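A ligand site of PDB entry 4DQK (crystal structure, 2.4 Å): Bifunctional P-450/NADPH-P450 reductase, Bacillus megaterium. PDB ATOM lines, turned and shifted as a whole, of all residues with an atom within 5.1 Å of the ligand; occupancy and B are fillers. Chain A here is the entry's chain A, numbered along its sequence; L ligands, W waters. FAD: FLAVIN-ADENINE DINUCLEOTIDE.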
ATOM      1  N   HIS A  42      -2.957  -7.901  24.638  1.00  0.00           N
ATOM      2  CA  HIS A  42      -2.975  -8.052  23.182  1.00  0.00           C
ATOM      3  C   HIS A  42      -1.606  -8.321  22.632  1.00  0.00           C
ATOM      4  O   HIS A  42      -0.579  -7.813  23.170  1.00  0.00           O
ATOM      5  CB  HIS A  42      -3.497  -6.798  22.529  1.00  0.00           C
ATOM      6  CG  HIS A  42      -4.885  -6.445  22.931  1.00  0.00           C
ATOM      7  ND1 HIS A  42      -5.179  -5.375  23.740  1.00  0.00           N
ATOM      8  CD2 HIS A  42      -6.060  -7.014  22.633  1.00  0.00           C
ATOM      9  CE1 HIS A  42      -6.475  -5.316  23.916  1.00  0.00           C
ATOM     10  NE2 HIS A  42      -7.035  -6.319  23.282  1.00  0.00           N
ATOM     11  N   GLN A  99      -3.083  -0.542   1.067  1.00  0.00           N
ATOM     12  CA  GLN A  99      -4.511  -0.488   0.843  1.00  0.00           C
ATOM     13  C   GLN A  99      -5.334   0.374   1.780  1.00  0.00           C
ATOM     14  O   GLN A  99      -6.531   0.084   2.051  1.00  0.00           O
ATOM     15  CB  GLN A  99      -5.116  -1.889   0.634  1.00  0.00           C
ATOM     16  CG  GLN A  99      -5.094  -2.780   1.786  1.00  0.00           C
ATOM     17  CD  GLN A  99      -5.627  -4.173   1.496  1.00  0.00           C
ATOM     18  OE1 GLN A  99      -5.667  -4.660   0.336  1.00  0.00           O
ATOM     19  NE2 GLN A  99      -5.990  -4.872   2.597  1.00  0.00           N
ATOM     20  N   LYS A 139     -15.910   3.455   0.042  1.00  0.00           N
ATOM     21  CA  LYS A 139     -15.577   2.239  -0.683  1.00  0.00           C
ATOM     22  C   LYS A 139     -14.160   1.829  -0.483  1.00  0.00           C
ATOM     23  O   LYS A 139     -13.715   0.848  -0.993  1.00  0.00           O
ATOM     24  CB  LYS A 139     -15.754   2.536  -2.134  1.00  0.00           C
ATOM     25  CG  LYS A 139     -17.219   2.760  -2.520  1.00  0.00           C
ATOM     26  CD  LYS A 139     -17.267   3.450  -3.823  1.00  0.00           C
ATOM     27  CE  LYS A 139     -17.009   2.541  -5.049  1.00  0.00           C
ATOM     28  NZ  LYS A 139     -17.098   3.484  -6.295  1.00  0.00           N
ATOM     29  N   ARG A 140     -13.424   2.587   0.297  1.00  0.00           N
ATOM     30  CA  ARG A 140     -12.034   2.298   0.528  1.00  0.00           C
ATOM     31  C   ARG A 140     -11.181   2.122  -0.769  1.00  0.00           C
ATOM     32  O   ARG A 140     -10.396   1.156  -0.941  1.00  0.00           O
ATOM     33  CB  ARG A 140     -11.919   1.126   1.451  1.00  0.00           C
ATOM     34  CG  ARG A 140     -12.295   1.509   2.894  1.00  0.00           C
ATOM     35  CD  ARG A 140     -12.208   0.319   3.783  1.00  0.00           C
ATOM     36  NE  ARG A 140     -10.965  -0.435   3.619  1.00  0.00           N
ATOM     37  CZ  ARG A 140      -9.847  -0.143   4.253  1.00  0.00           C
ATOM     38  NH1 ARG A 140      -9.784   0.957   5.018  1.00  0.00           N
ATOM     39  NH2 ARG A 140      -8.782  -0.940   4.117  1.00  0.00           N
ATOM     40  N   ARG A 170      -1.122  -4.665  13.876  1.00  0.00           N
ATOM     41  CA  ARG A 170      -2.461  -5.116  14.134  1.00  0.00           C
ATOM     42  C   ARG A 170      -2.513  -5.827  15.474  1.00  0.00           C
ATOM     43  O   ARG A 170      -1.588  -6.500  15.837  1.00  0.00           O
ATOM     44  CB  ARG A 170      -3.038  -5.894  12.932  1.00  0.00           C
ATOM     45  CG  ARG A 170      -3.970  -4.948  12.150  1.00  0.00           C
ATOM     46  CD  ARG A 170      -3.819  -4.806  10.598  1.00  0.00           C
ATOM     47  NE  ARG A 170      -2.686  -4.066  10.213  1.00  0.00           N
ATOM     48  CZ  ARG A 170      -2.499  -3.434   9.041  1.00  0.00           C
ATOM     49  NH1 ARG A 170      -3.355  -3.501   8.053  1.00  0.00           N
ATOM     50  NH2 ARG A 170      -1.369  -2.727   8.884  1.00  0.00           N
ATOM     51  N   TYR A 171      -3.597  -5.573  16.238  1.00  0.00           N
ATOM     52  CA  TYR A 171      -3.738  -6.136  17.570  1.00  0.00           C
ATOM     53  C   TYR A 171      -4.644  -7.332  17.586  1.00  0.00           C
ATOM     54  O   TYR A 171      -5.684  -7.330  16.933  1.00  0.00           O
ATOM     55  CB  TYR A 171      -4.206  -5.085  18.540  1.00  0.00           C
ATOM     56  CG  TYR A 171      -3.198  -3.963  18.602  1.00  0.00           C
ATOM     57  CD1 TYR A 171      -3.299  -2.834  17.759  1.00  0.00           C
ATOM     58  CD2 TYR A 171      -2.133  -4.030  19.426  1.00  0.00           C
ATOM     59  CE1 TYR A 171      -2.368  -1.793  17.809  1.00  0.00           C
ATOM     60  CE2 TYR A 171      -1.165  -2.980  19.445  1.00  0.00           C
ATOM     61  CZ  TYR A 171      -1.297  -1.883  18.630  1.00  0.00           C
ATOM     62  OH  TYR A 171      -0.335  -0.839  18.681  1.00  0.00           O
ATOM     63  N   TYR A 172      -4.188  -8.359  18.290  1.00  0.00           N
ATOM     64  CA  TYR A 172      -4.965  -9.540  18.535  1.00  0.00           C
ATOM     65  C   TYR A 172      -5.067  -9.921  20.063  1.00  0.00           C
ATOM     66  O   TYR A 172      -4.093  -9.924  20.824  1.00  0.00           O
ATOM     67  CB  TYR A 172      -4.370 -10.679  17.693  1.00  0.00           C
ATOM     68  CG  TYR A 172      -4.480 -10.359  16.255  1.00  0.00           C
ATOM     69  CD1 TYR A 172      -5.655 -10.576  15.564  1.00  0.00           C
ATOM     70  CD2 TYR A 172      -3.457  -9.721  15.596  1.00  0.00           C
ATOM     71  CE1 TYR A 172      -5.792 -10.199  14.221  1.00  0.00           C
ATOM     72  CE2 TYR A 172      -3.596  -9.340  14.303  1.00  0.00           C
ATOM     73  CZ  TYR A 172      -4.761  -9.564  13.620  1.00  0.00           C
ATOM     74  OH  TYR A 172      -4.841  -9.216  12.280  1.00  0.00           O
ATOM     75  N   SER A 173      -6.255 -10.240  20.493  1.00  0.00           N
ATOM     76  CA  SER A 173      -6.500 -10.566  21.896  1.00  0.00           C
ATOM     77  C   SER A 173      -5.925 -11.902  22.174  1.00  0.00           C
ATOM     78  O   SER A 173      -6.385 -12.886  21.642  1.00  0.00           O
ATOM     79  CB  SER A 173      -8.000 -10.660  22.114  1.00  0.00           C
ATOM     80  OG  SER A 173      -8.589  -9.427  21.795  1.00  0.00           O
ATOM     81  N   THR A 188      -6.286 -15.689  17.980  1.00  0.00           N
ATOM     82  CA  THR A 188      -7.414 -16.253  17.304  1.00  0.00           C
ATOM     83  C   THR A 188      -7.876 -15.239  16.296  1.00  0.00           C
ATOM     84  O   THR A 188      -8.405 -14.195  16.660  1.00  0.00           O
ATOM     85  CB  THR A 188      -8.529 -16.580  18.376  1.00  0.00           C
ATOM     86  OG1 THR A 188      -7.950 -17.406  19.404  1.00  0.00           O
ATOM     87  CG2 THR A 188      -9.727 -17.246  17.758  1.00  0.00           C
ATOM     88  N   VAL A 189      -7.704 -15.566  15.003  1.00  0.00           N
ATOM     89  CA  VAL A 189      -7.648 -14.548  13.964  1.00  0.00           C
ATOM     90  C   VAL A 189      -8.644 -14.770  12.895  1.00  0.00           C
ATOM     91  O   VAL A 189      -8.514 -15.685  12.121  1.00  0.00           O
ATOM     92  CB  VAL A 189      -6.223 -14.561  13.290  1.00  0.00           C
ATOM     93  CG1 VAL A 189      -6.145 -13.468  12.178  1.00  0.00           C
ATOM     94  CG2 VAL A 189      -5.178 -14.313  14.314  1.00  0.00           C
ATOM     95  N   SER A 190      -9.654 -13.943  12.823  1.00  0.00           N
ATOM     96  CA  SER A 190     -10.609 -14.098  11.747  1.00  0.00           C
ATOM     97  C   SER A 190      -9.988 -13.535  10.407  1.00  0.00           C
ATOM     98  O   SER A 190      -9.418 -12.377  10.381  1.00  0.00           O
ATOM     99  CB  SER A 190     -11.904 -13.393  12.166  1.00  0.00           C
ATOM    100  OG  SER A 190     -12.554 -12.804  11.064  1.00  0.00           O
ATOM    101  N   VAL A 192      -9.836 -11.824   7.030  1.00  0.00           N
ATOM    102  CA  VAL A 192     -10.599 -10.854   6.256  1.00  0.00           C
ATOM    103  C   VAL A 192     -10.408 -11.131   4.758  1.00  0.00           C
ATOM    104  O   VAL A 192      -9.278 -11.248   4.221  1.00  0.00           O
ATOM    105  CB  VAL A 192     -10.329  -9.374   6.672  1.00  0.00           C
ATOM    106  CG1 VAL A 192     -11.170  -8.329   5.771  1.00  0.00           C
ATOM    107  CG2 VAL A 192     -10.727  -9.150   8.146  1.00  0.00           C
ATOM    108  N   GLY A 194     -13.065 -11.001   0.893  1.00  0.00           N
ATOM    109  CA  GLY A 194     -14.363 -10.706   0.247  1.00  0.00           C
ATOM    110  C   GLY A 194     -14.157 -10.000  -1.091  1.00  0.00           C
ATOM    111  O   GLY A 194     -13.051  -9.935  -1.583  1.00  0.00           O
ATOM    112  N   GLU A 195     -15.225  -9.542  -1.691  1.00  0.00           N
ATOM    113  CA  GLU A 195     -15.129  -8.721  -2.857  1.00  0.00           C
ATOM    114  C   GLU A 195     -14.815  -7.317  -2.337  1.00  0.00           C
ATOM    115  O   GLU A 195     -15.523  -6.832  -1.443  1.00  0.00           O
ATOM    116  CB  GLU A 195     -16.453  -8.731  -3.682  1.00  0.00           C
ATOM    117  CG  GLU A 195     -16.716 -10.048  -4.576  1.00  0.00           C
ATOM    118  N   ALA A 196     -13.788  -6.674  -2.910  1.00  0.00           N
ATOM    119  CA  ALA A 196     -13.434  -5.319  -2.541  1.00  0.00           C
ATOM    120  C   ALA A 196     -14.586  -4.359  -2.689  1.00  0.00           C
ATOM    121  O   ALA A 196     -15.214  -4.283  -3.751  1.00  0.00           O
ATOM    122  CB  ALA A 196     -12.260  -4.859  -3.366  1.00  0.00           C
ATOM    123  N   TRP A 197     -14.855  -3.578  -1.661  1.00  0.00           N
ATOM    124  CA  TRP A 197     -15.924  -2.577  -1.775  1.00  0.00           C
ATOM    125  C   TRP A 197     -15.616  -1.540  -2.873  1.00  0.00           C
ATOM    126  O   TRP A 197     -16.507  -0.791  -3.296  1.00  0.00           O
ATOM    127  CB  TRP A 197     -16.168  -1.793  -0.451  1.00  0.00           C
ATOM    128  CG  TRP A 197     -16.426  -2.593   0.712  1.00  0.00           C
ATOM    129  CD1 TRP A 197     -16.878  -3.900   0.733  1.00  0.00           C
ATOM    130  CD2 TRP A 197     -16.181  -2.224   2.072  1.00  0.00           C
ATOM    131  NE1 TRP A 197     -16.886  -4.348   2.001  1.00  0.00           N
ATOM    132  CE2 TRP A 197     -16.485  -3.336   2.862  1.00  0.00           C
ATOM    133  CE3 TRP A 197     -15.756  -1.056   2.711  1.00  0.00           C
ATOM    134  CZ2 TRP A 197     -16.395  -3.311   4.259  1.00  0.00           C
ATOM    135  CZ3 TRP A 197     -15.633  -1.044   4.134  1.00  0.00           C
ATOM    136  CH2 TRP A 197     -15.958  -2.155   4.854  1.00  0.00           C
ATOM    137  N   TYR A 203     -10.578  -8.553  -2.225  1.00  0.00           N
ATOM    138  CA  TYR A 203      -9.949  -7.952  -1.089  1.00  0.00           C
ATOM    139  C   TYR A 203      -9.427  -8.980  -0.081  1.00  0.00           C
ATOM    140  O   TYR A 203     -10.118  -9.968   0.247  1.00  0.00           O
ATOM    141  CB  TYR A 203     -10.940  -7.053  -0.430  1.00  0.00           C
ATOM    142  CG  TYR A 203     -10.350  -6.212   0.646  1.00  0.00           C
ATOM    143  CD1 TYR A 203      -9.802  -4.994   0.339  1.00  0.00           C
ATOM    144  CD2 TYR A 203     -10.328  -6.609   1.992  1.00  0.00           C
ATOM    145  CE1 TYR A 203      -9.279  -4.170   1.335  1.00  0.00           C
ATOM    146  CE2 TYR A 203      -9.783  -5.785   2.999  1.00  0.00           C
ATOM    147  CZ  TYR A 203      -9.251  -4.561   2.650  1.00  0.00           C
ATOM    148  OH  TYR A 203      -8.645  -3.717   3.561  1.00  0.00           O
ATOM    149  N   LYS A 204      -8.190  -8.791   0.376  1.00  0.00           N
ATOM    150  CA  LYS A 204      -7.633  -9.555   1.526  1.00  0.00           C
ATOM    151  C   LYS A 204      -7.042  -8.611   2.572  1.00  0.00           C
ATOM    152  O   LYS A 204      -6.286  -7.715   2.230  1.00  0.00           O
ATOM    153  CB  LYS A 204      -6.549 -10.516   1.084  1.00  0.00           C
ATOM    154  CG  LYS A 204      -7.071 -11.557   0.068  1.00  0.00           C
ATOM    155  CD  LYS A 204      -6.384 -12.860   0.090  1.00  0.00           C
ATOM    156  CE  LYS A 204      -4.863 -12.844  -0.107  1.00  0.00           C
ATOM    157  NZ  LYS A 204      -4.374 -14.121  -0.819  1.00  0.00           N
ATOM    158  N   GLY A 205      -7.410  -8.821   3.841  1.00  0.00           N
ATOM    159  CA  GLY A 205      -6.938  -7.965   4.943  1.00  0.00           C
ATOM    160  C   GLY A 205      -5.489  -8.264   5.165  1.00  0.00           C
ATOM    161  O   GLY A 205      -5.078  -9.430   5.179  1.00  0.00           O
ATOM    162  N   ILE A 206      -4.673  -7.223   5.339  1.00  0.00           N
ATOM    163  CA  ILE A 206      -3.236  -7.445   5.326  1.00  0.00           C
ATOM    164  C   ILE A 206      -2.778  -8.388   6.438  1.00  0.00           C
ATOM    165  O   ILE A 206      -2.293  -9.454   6.144  1.00  0.00           O
ATOM    166  CB  ILE A 206      -2.452  -6.067   5.323  1.00  0.00           C
ATOM    167  CG1 ILE A 206      -2.706  -5.273   4.036  1.00  0.00           C
ATOM    168  CG2 ILE A 206      -0.988  -6.311   5.449  1.00  0.00           C
ATOM    169  CD1 ILE A 206      -2.568  -6.005   2.691  1.00  0.00           C
ATOM    170  N   ALA A 207      -2.939  -8.039   7.708  1.00  0.00           N
ATOM    171  CA  ALA A 207      -2.344  -8.877   8.786  1.00  0.00           C
ATOM    172  C   ALA A 207      -3.035 -10.206   8.886  1.00  0.00           C
ATOM    173  O   ALA A 207      -2.415 -11.226   9.102  1.00  0.00           O
ATOM    174  CB  ALA A 207      -2.382  -8.148  10.114  1.00  0.00           C
ATOM    175  N   SER A 208      -4.334 -10.206   8.694  1.00  0.00           N
ATOM    176  CA  SER A 208      -5.050 -11.452   8.942  1.00  0.00           C
ATOM    177  C   SER A 208      -4.630 -12.524   7.949  1.00  0.00           C
ATOM    178  O   SER A 208      -4.513 -13.724   8.298  1.00  0.00           O
ATOM    179  CB  SER A 208      -6.561 -11.238   8.942  1.00  0.00           C
ATOM    180  OG  SER A 208      -7.050 -10.569   7.800  1.00  0.00           O
ATOM    181  N   ASN A 209      -4.391 -12.118   6.692  1.00  0.00           N
ATOM    182  CA  ASN A 209      -3.956 -13.111   5.642  1.00  0.00           C
ATOM    183  C   ASN A 209      -2.485 -13.399   5.799  1.00  0.00           C
ATOM    184  O   ASN A 209      -2.011 -14.463   5.566  1.00  0.00           O
ATOM    185  CB  ASN A 209      -4.333 -12.601   4.264  1.00  0.00           C
ATOM    186  CG  ASN A 209      -5.798 -12.836   3.918  1.00  0.00           C
ATOM    187  OD1 ASN A 209      -6.078 -13.903   3.443  1.00  0.00           O
ATOM    188  ND2 ASN A 209      -6.716 -11.865   4.157  1.00  0.00           N
ATOM    189  N   THR A 248     -14.907 -14.630  16.985  1.00  0.00           N
ATOM    190  CA  THR A 248     -13.545 -14.470  17.418  1.00  0.00           C
ATOM    191  C   THR A 248     -13.574 -13.728  18.719  1.00  0.00           C
ATOM    192  O   THR A 248     -12.593 -13.637  19.421  1.00  0.00           O
ATOM    193  CB  THR A 248     -12.816 -13.590  16.298  1.00  0.00           C
ATOM    194  OG1 THR A 248     -13.244 -14.078  15.012  1.00  0.00           O
ATOM    195  CG2 THR A 248     -11.355 -13.667  16.352  1.00  0.00           C
ATOM    196  N   ALA A 251     -12.086 -15.096  21.981  1.00  0.00           N
ATOM    197  CA  ALA A 251     -10.632 -15.190  22.143  1.00  0.00           C
ATOM    198  C   ALA A 251     -10.198 -14.975  23.575  1.00  0.00           C
ATOM    199  O   ALA A 251      -9.665 -15.865  24.161  1.00  0.00           O
ATOM    200  CB  ALA A 251      -9.852 -14.204  21.182  1.00  0.00           C
ATOM    201  N   ASP A 387     -13.615  -5.603  25.357  1.00  0.00           N
ATOM    202  CA  ASP A 387     -12.497  -5.818  24.439  1.00  0.00           C
ATOM    203  C   ASP A 387     -13.054  -5.965  23.008  1.00  0.00           C
ATOM    204  O   ASP A 387     -13.039  -7.008  22.429  1.00  0.00           O
ATOM    205  CB  ASP A 387     -11.688  -7.059  24.873  1.00  0.00           C
ATOM    206  CG  ASP A 387     -10.518  -7.368  23.928  1.00  0.00           C
ATOM    207  OD1 ASP A 387      -9.746  -6.390  23.602  1.00  0.00           O
ATOM    208  OD2 ASP A 387     -10.378  -8.578  23.547  1.00  0.00           O
ATOM    209  N   VAL A 388     -13.619  -4.907  22.494  1.00  0.00           N
ATOM    210  CA  VAL A 388     -14.304  -4.995  21.236  1.00  0.00           C
ATOM    211  C   VAL A 388     -13.552  -4.185  20.141  1.00  0.00           C
ATOM    212  O   VAL A 388     -12.790  -3.256  20.424  1.00  0.00           O
ATOM    213  CB  VAL A 388     -15.759  -4.447  21.373  1.00  0.00           C
ATOM    214  CG1 VAL A 388     -16.565  -5.269  22.392  1.00  0.00           C
ATOM    215  CG2 VAL A 388     -15.757  -2.883  21.688  1.00  0.00           C
ATOM    216  N   TRP A 389     -13.850  -4.476  18.892  1.00  0.00           N
ATOM    217  CA  TRP A 389     -13.190  -3.845  17.794  1.00  0.00           C
ATOM    218  C   TRP A 389     -14.108  -3.732  16.602  1.00  0.00           C
ATOM    219  O   TRP A 389     -15.152  -4.342  16.546  1.00  0.00           O
ATOM    220  CB  TRP A 389     -11.885  -4.597  17.428  1.00  0.00           C
ATOM    221  CG  TRP A 389     -12.012  -6.051  17.045  1.00  0.00           C
ATOM    222  CD1 TRP A 389     -12.157  -6.549  15.813  1.00  0.00           C
ATOM    223  CD2 TRP A 389     -11.958  -7.175  17.918  1.00  0.00           C
ATOM    224  NE1 TRP A 389     -12.224  -7.948  15.841  1.00  0.00           N
ATOM    225  CE2 TRP A 389     -12.128  -8.345  17.137  1.00  0.00           C
ATOM    226  CE3 TRP A 389     -11.856  -7.316  19.305  1.00  0.00           C
ATOM    227  CZ2 TRP A 389     -12.165  -9.603  17.681  1.00  0.00           C
ATOM    228  CZ3 TRP A 389     -11.854  -8.585  19.852  1.00  0.00           C
ATOM    229  CH2 TRP A 389     -11.992  -9.717  19.034  1.00  0.00           C
HETATM  230  PA  FAD L   1      -6.784  -4.634   6.891  1.00  0.00           P
HETATM  231  O1A FAD L   1      -5.867  -4.817   5.753  1.00  0.00           O
HETATM  232  O2A FAD L   1      -6.367  -3.636   7.943  1.00  0.00           O
HETATM  233  O5B FAD L   1      -8.214  -4.120   6.414  1.00  0.00           O
HETATM  234  C5B FAD L   1      -9.088  -3.772   7.442  1.00  0.00           C
HETATM  235  C4B FAD L   1     -10.138  -2.879   6.892  1.00  0.00           C
HETATM  236  O4B FAD L   1     -10.689  -3.453   5.700  1.00  0.00           O
HETATM  237  C3B FAD L   1     -11.278  -2.685   7.893  1.00  0.00           C
HETATM  238  O3B FAD L   1     -11.622  -1.311   7.748  1.00  0.00           O
HETATM  239  C2B FAD L   1     -12.401  -3.456   7.276  1.00  0.00           C
HETATM  240  O2B FAD L   1     -13.653  -2.881   7.516  1.00  0.00           O
HETATM  241  C1B FAD L   1     -12.093  -3.308   5.745  1.00  0.00           C
HETATM  242  N9A FAD L   1     -12.758  -4.284   4.860  1.00  0.00           N
HETATM  243  C8A FAD L   1     -13.298  -5.474   5.196  1.00  0.00           C
HETATM  244  N7A FAD L   1     -13.818  -6.037   4.127  1.00  0.00           N
HETATM  245  C5A FAD L   1     -13.576  -5.297   3.069  1.00  0.00           C
HETATM  246  C6A FAD L   1     -13.875  -5.462   1.734  1.00  0.00           C
HETATM  247  N6A FAD L   1     -14.452  -6.562   1.300  1.00  0.00           N
HETATM  248  N1A FAD L   1     -13.521  -4.485   0.810  1.00  0.00           N
HETATM  249  C2A FAD L   1     -12.885  -3.407   1.311  1.00  0.00           C
HETATM  250  N3A FAD L   1     -12.596  -3.235   2.639  1.00  0.00           N
HETATM  251  C4A FAD L   1     -12.913  -4.192   3.516  1.00  0.00           C
HETATM  252  N1  FAD L   1      -9.148  -9.461  15.082  1.00  0.00           N
HETATM  253  C2  FAD L   1      -9.201 -10.832  15.235  1.00  0.00           C
HETATM  254  O2  FAD L   1      -9.410 -11.609  14.302  1.00  0.00           O
HETATM  255  N3  FAD L   1      -8.970 -11.398  16.454  1.00  0.00           N
HETATM  256  C4  FAD L   1      -8.806 -10.604  17.553  1.00  0.00           C
HETATM  257  O4  FAD L   1      -8.603 -11.148  18.633  1.00  0.00           O
HETATM  258  C4X FAD L   1      -8.778  -9.241  17.444  1.00  0.00           C
HETATM  259  N5  FAD L   1      -8.578  -8.463  18.591  1.00  0.00           N
HETATM  260  C5X FAD L   1      -8.522  -7.094  18.461  1.00  0.00           C
HETATM  261  C6  FAD L   1      -8.280  -6.279  19.571  1.00  0.00           C
HETATM  262  C7  FAD L   1      -8.295  -4.891  19.420  1.00  0.00           C
HETATM  263  C7M FAD L   1      -8.083  -3.939  20.593  1.00  0.00           C
HETATM  264  C8  FAD L   1      -8.396  -4.309  18.158  1.00  0.00           C
HETATM  265  C8M FAD L   1      -8.368  -2.757  17.979  1.00  0.00           C
HETATM  266  C9  FAD L   1      -8.556  -5.155  17.084  1.00  0.00           C
HETATM  267  C9A FAD L   1      -8.644  -6.522  17.205  1.00  0.00           C
HETATM  268  N10 FAD L   1      -8.855  -7.318  16.071  1.00  0.00           N
HETATM  269  C10 FAD L   1      -8.900  -8.670  16.189  1.00  0.00           C
HETATM  270  C1' FAD L   1      -8.981  -6.717  14.692  1.00  0.00           C
HETATM  271  C2' FAD L   1      -7.532  -6.862  14.124  1.00  0.00           C
HETATM  272  O2' FAD L   1      -6.584  -6.062  14.767  1.00  0.00           O
HETATM  273  C3' FAD L   1      -7.360  -6.501  12.675  1.00  0.00           C
HETATM  274  O3' FAD L   1      -7.909  -5.239  12.526  1.00  0.00           O
HETATM  275  C4' FAD L   1      -8.109  -7.424  11.720  1.00  0.00           C
HETATM  276  O4' FAD L   1      -7.471  -8.659  11.751  1.00  0.00           O
HETATM  277  C5' FAD L   1      -8.055  -6.825  10.308  1.00  0.00           C
HETATM  278  O5' FAD L   1      -6.770  -6.302   9.956  1.00  0.00           O
HETATM  279  P   FAD L   1      -6.151  -6.791   8.542  1.00  0.00           P
HETATM  280  O1P FAD L   1      -4.799  -6.159   8.375  1.00  0.00           O
HETATM  281  O2P FAD L   1      -6.253  -8.293   8.247  1.00  0.00           O
HETATM  282  O3P FAD L   1      -7.056  -6.132   7.435  1.00  0.00           O
HETATM  283  O   HOH W   1      -6.576  -0.793   7.940  1.00  0.00           O
HETATM  284  O   HOH W   2      -5.797  -1.663   5.153  1.00  0.00           O
HETATM  285  O   HOH W   3      -9.400 -10.377  12.026  1.00  0.00           O
HETATM  286  O   HOH W   4      -6.902 -13.213  19.029  1.00  0.00           O
HETATM  287  O   HOH W   5      -5.648  -3.680  15.062  1.00  0.00           O
HETATM  288  O   HOH W   6     -16.758  -8.386   2.388  1.00  0.00           O
HETATM  289  O   HOH W   7      -6.888  -3.284  10.641  1.00  0.00           O
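An oxygen (O1P) of the ligand is in hydrogen-bond range of the backbone NH of Ala 207 (2.7 Å).
An oxygen (O4') of the ligand lies within hydrogen-bond range of the side-chain hydroxyl (OH) of Tyr 172, at 2.7 Å.
The backbone NH (N) of Ser 173 sits at hydrogen-bond distance from an oxygen (O4) of the ligand.
O of Tyr 171 is in hydrogen-bond range of O2' of the ligand (2.7 Å).
The side-chain hydroxyl of Ser 173 lies within hydrogen-bond range of a nitrogen (N5) of the ligand (3.3 Å).
A nitrogen (N3) of the ligand is in hydrogen-bond range of the backbone carbonyl oxygen (O) of Thr 188 (2.9 Å).
The guanidinium group (NH1) of Arg 170 is in salt-bridge range of an oxygen (O2A) of the ligand, 3.0 Å away.
OH of Tyr 203 sits at hydrogen-bond distance from O5B of the ligand, at 2.9 Å.
N of Tyr 171 lies within hydrogen-bond range of O2' of the ligand, at 3.4 Å.
The backbone NH of Ile 206 lies within hydrogen-bond range of an oxygen (O1A) of the ligand, at 2.7 Å.
O1A of the ligand sits at hydrogen-bond distance from NE2 of Gln 99 (3.2 Å).
N1A of the ligand sits at hydrogen-bond distance from N of Trp 197.
O2P of the ligand sits at hydrogen-bond distance from N of Ser 208, at 2.7 Å.
A nitrogen (N3A) of the ligand lies within hydrogen-bond range of the guanidinium group (NE) of Arg 140 (3.4 Å).
A nitrogen (N6A) of the ligand is in hydrogen-bond range of the backbone carbonyl oxygen (O) of Glu 195 (3.0 Å).
The side-chain hydroxyl (OG) of Ser 208 is in hydrogen-bond range of an oxygen (O2P) of the ligand (2.5 Å).
The backbone NH of Ser 190 is in hydrogen-bond range of an oxygen (O2) of the ligand.
NE2 of Gln 99 sits at hydrogen-bond distance from OH of Tyr 203 (3.1 Å).
The guanidinium group (NH2) of Arg 140 lies within hydrogen-bond range of the side-chain hydroxyl (OH) of Tyr 203 (2.8 Å).
The backbone carbonyl oxygen (O) of Gly 205 sits at hydrogen-bond distance from the side-chain amide nitrogen (ND2) of Asn 209, at 3.1 Å.
The side-chain carboxylate of Asp 387 lies within hydrogen-bond range of a ring nitrogen (NE2) of His 42, 2.7 Å away.
The guanidinium group of Arg 140 sits at hydrogen-bond distance from the backbone carbonyl oxygen of Gln 99, 3.2 Å away.
O of Val 192 lies within hydrogen-bond range of N of Gly 205.
OD2 of Asp 387 sits at hydrogen-bond distance from OG of Ser 173, 2.6 Å away.
OG of Ser 208 lies within hydrogen-bond range of N of Val 192, 3.2 Å away.
An oxygen (O2P) of the ligand sits close to the backbone carbonyl oxygen (O) of Gly 205 (3.5 Å).
NE1 of Trp 389 lies close to N10 of the ligand (3.4 Å).
Residues that only touch the ligand: His 42 (3.7 Å), Val 189 (3.4 Å), Val 192 (3.6 Å), Ala 196 (3.5 Å) and Thr 248 (3.3 Å).
Hydrophobic or aromatic side chains that line the ligand: His 42, Tyr 172, Val 192, Trp 197, Tyr 203, Ile 206, Ala 207 and Trp 389.
21 residues have an atom within 4 Å of the ligand: His 42, Gln 99, Arg 140, Arg 170, Tyr 171, Tyr 172, Ser 173, Thr 188, Val 189, Ser 190, Val 192, Glu 195, Ala 196, Trp 197, Tyr 203, Gly 205, Ile 206, Ala 207, Ser 208, Thr 248 and Trp 389.
Water W5 bridges O2' of the ligand (2.6 Å) and N of Tyr 171 (3.0 Å).
Water W3 lies within hydrogen-bond range of an oxygen (O2) of the ligand (2.6 Å) and the backbone carbonyl oxygen of Ser 190 (2.6 Å).
Water W4 lies within hydrogen-bond range of O of Ser 173, O4 of the ligand and N of Thr 188.
Water W2 bridges O1A of the ligand and NH2 of Arg 140.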
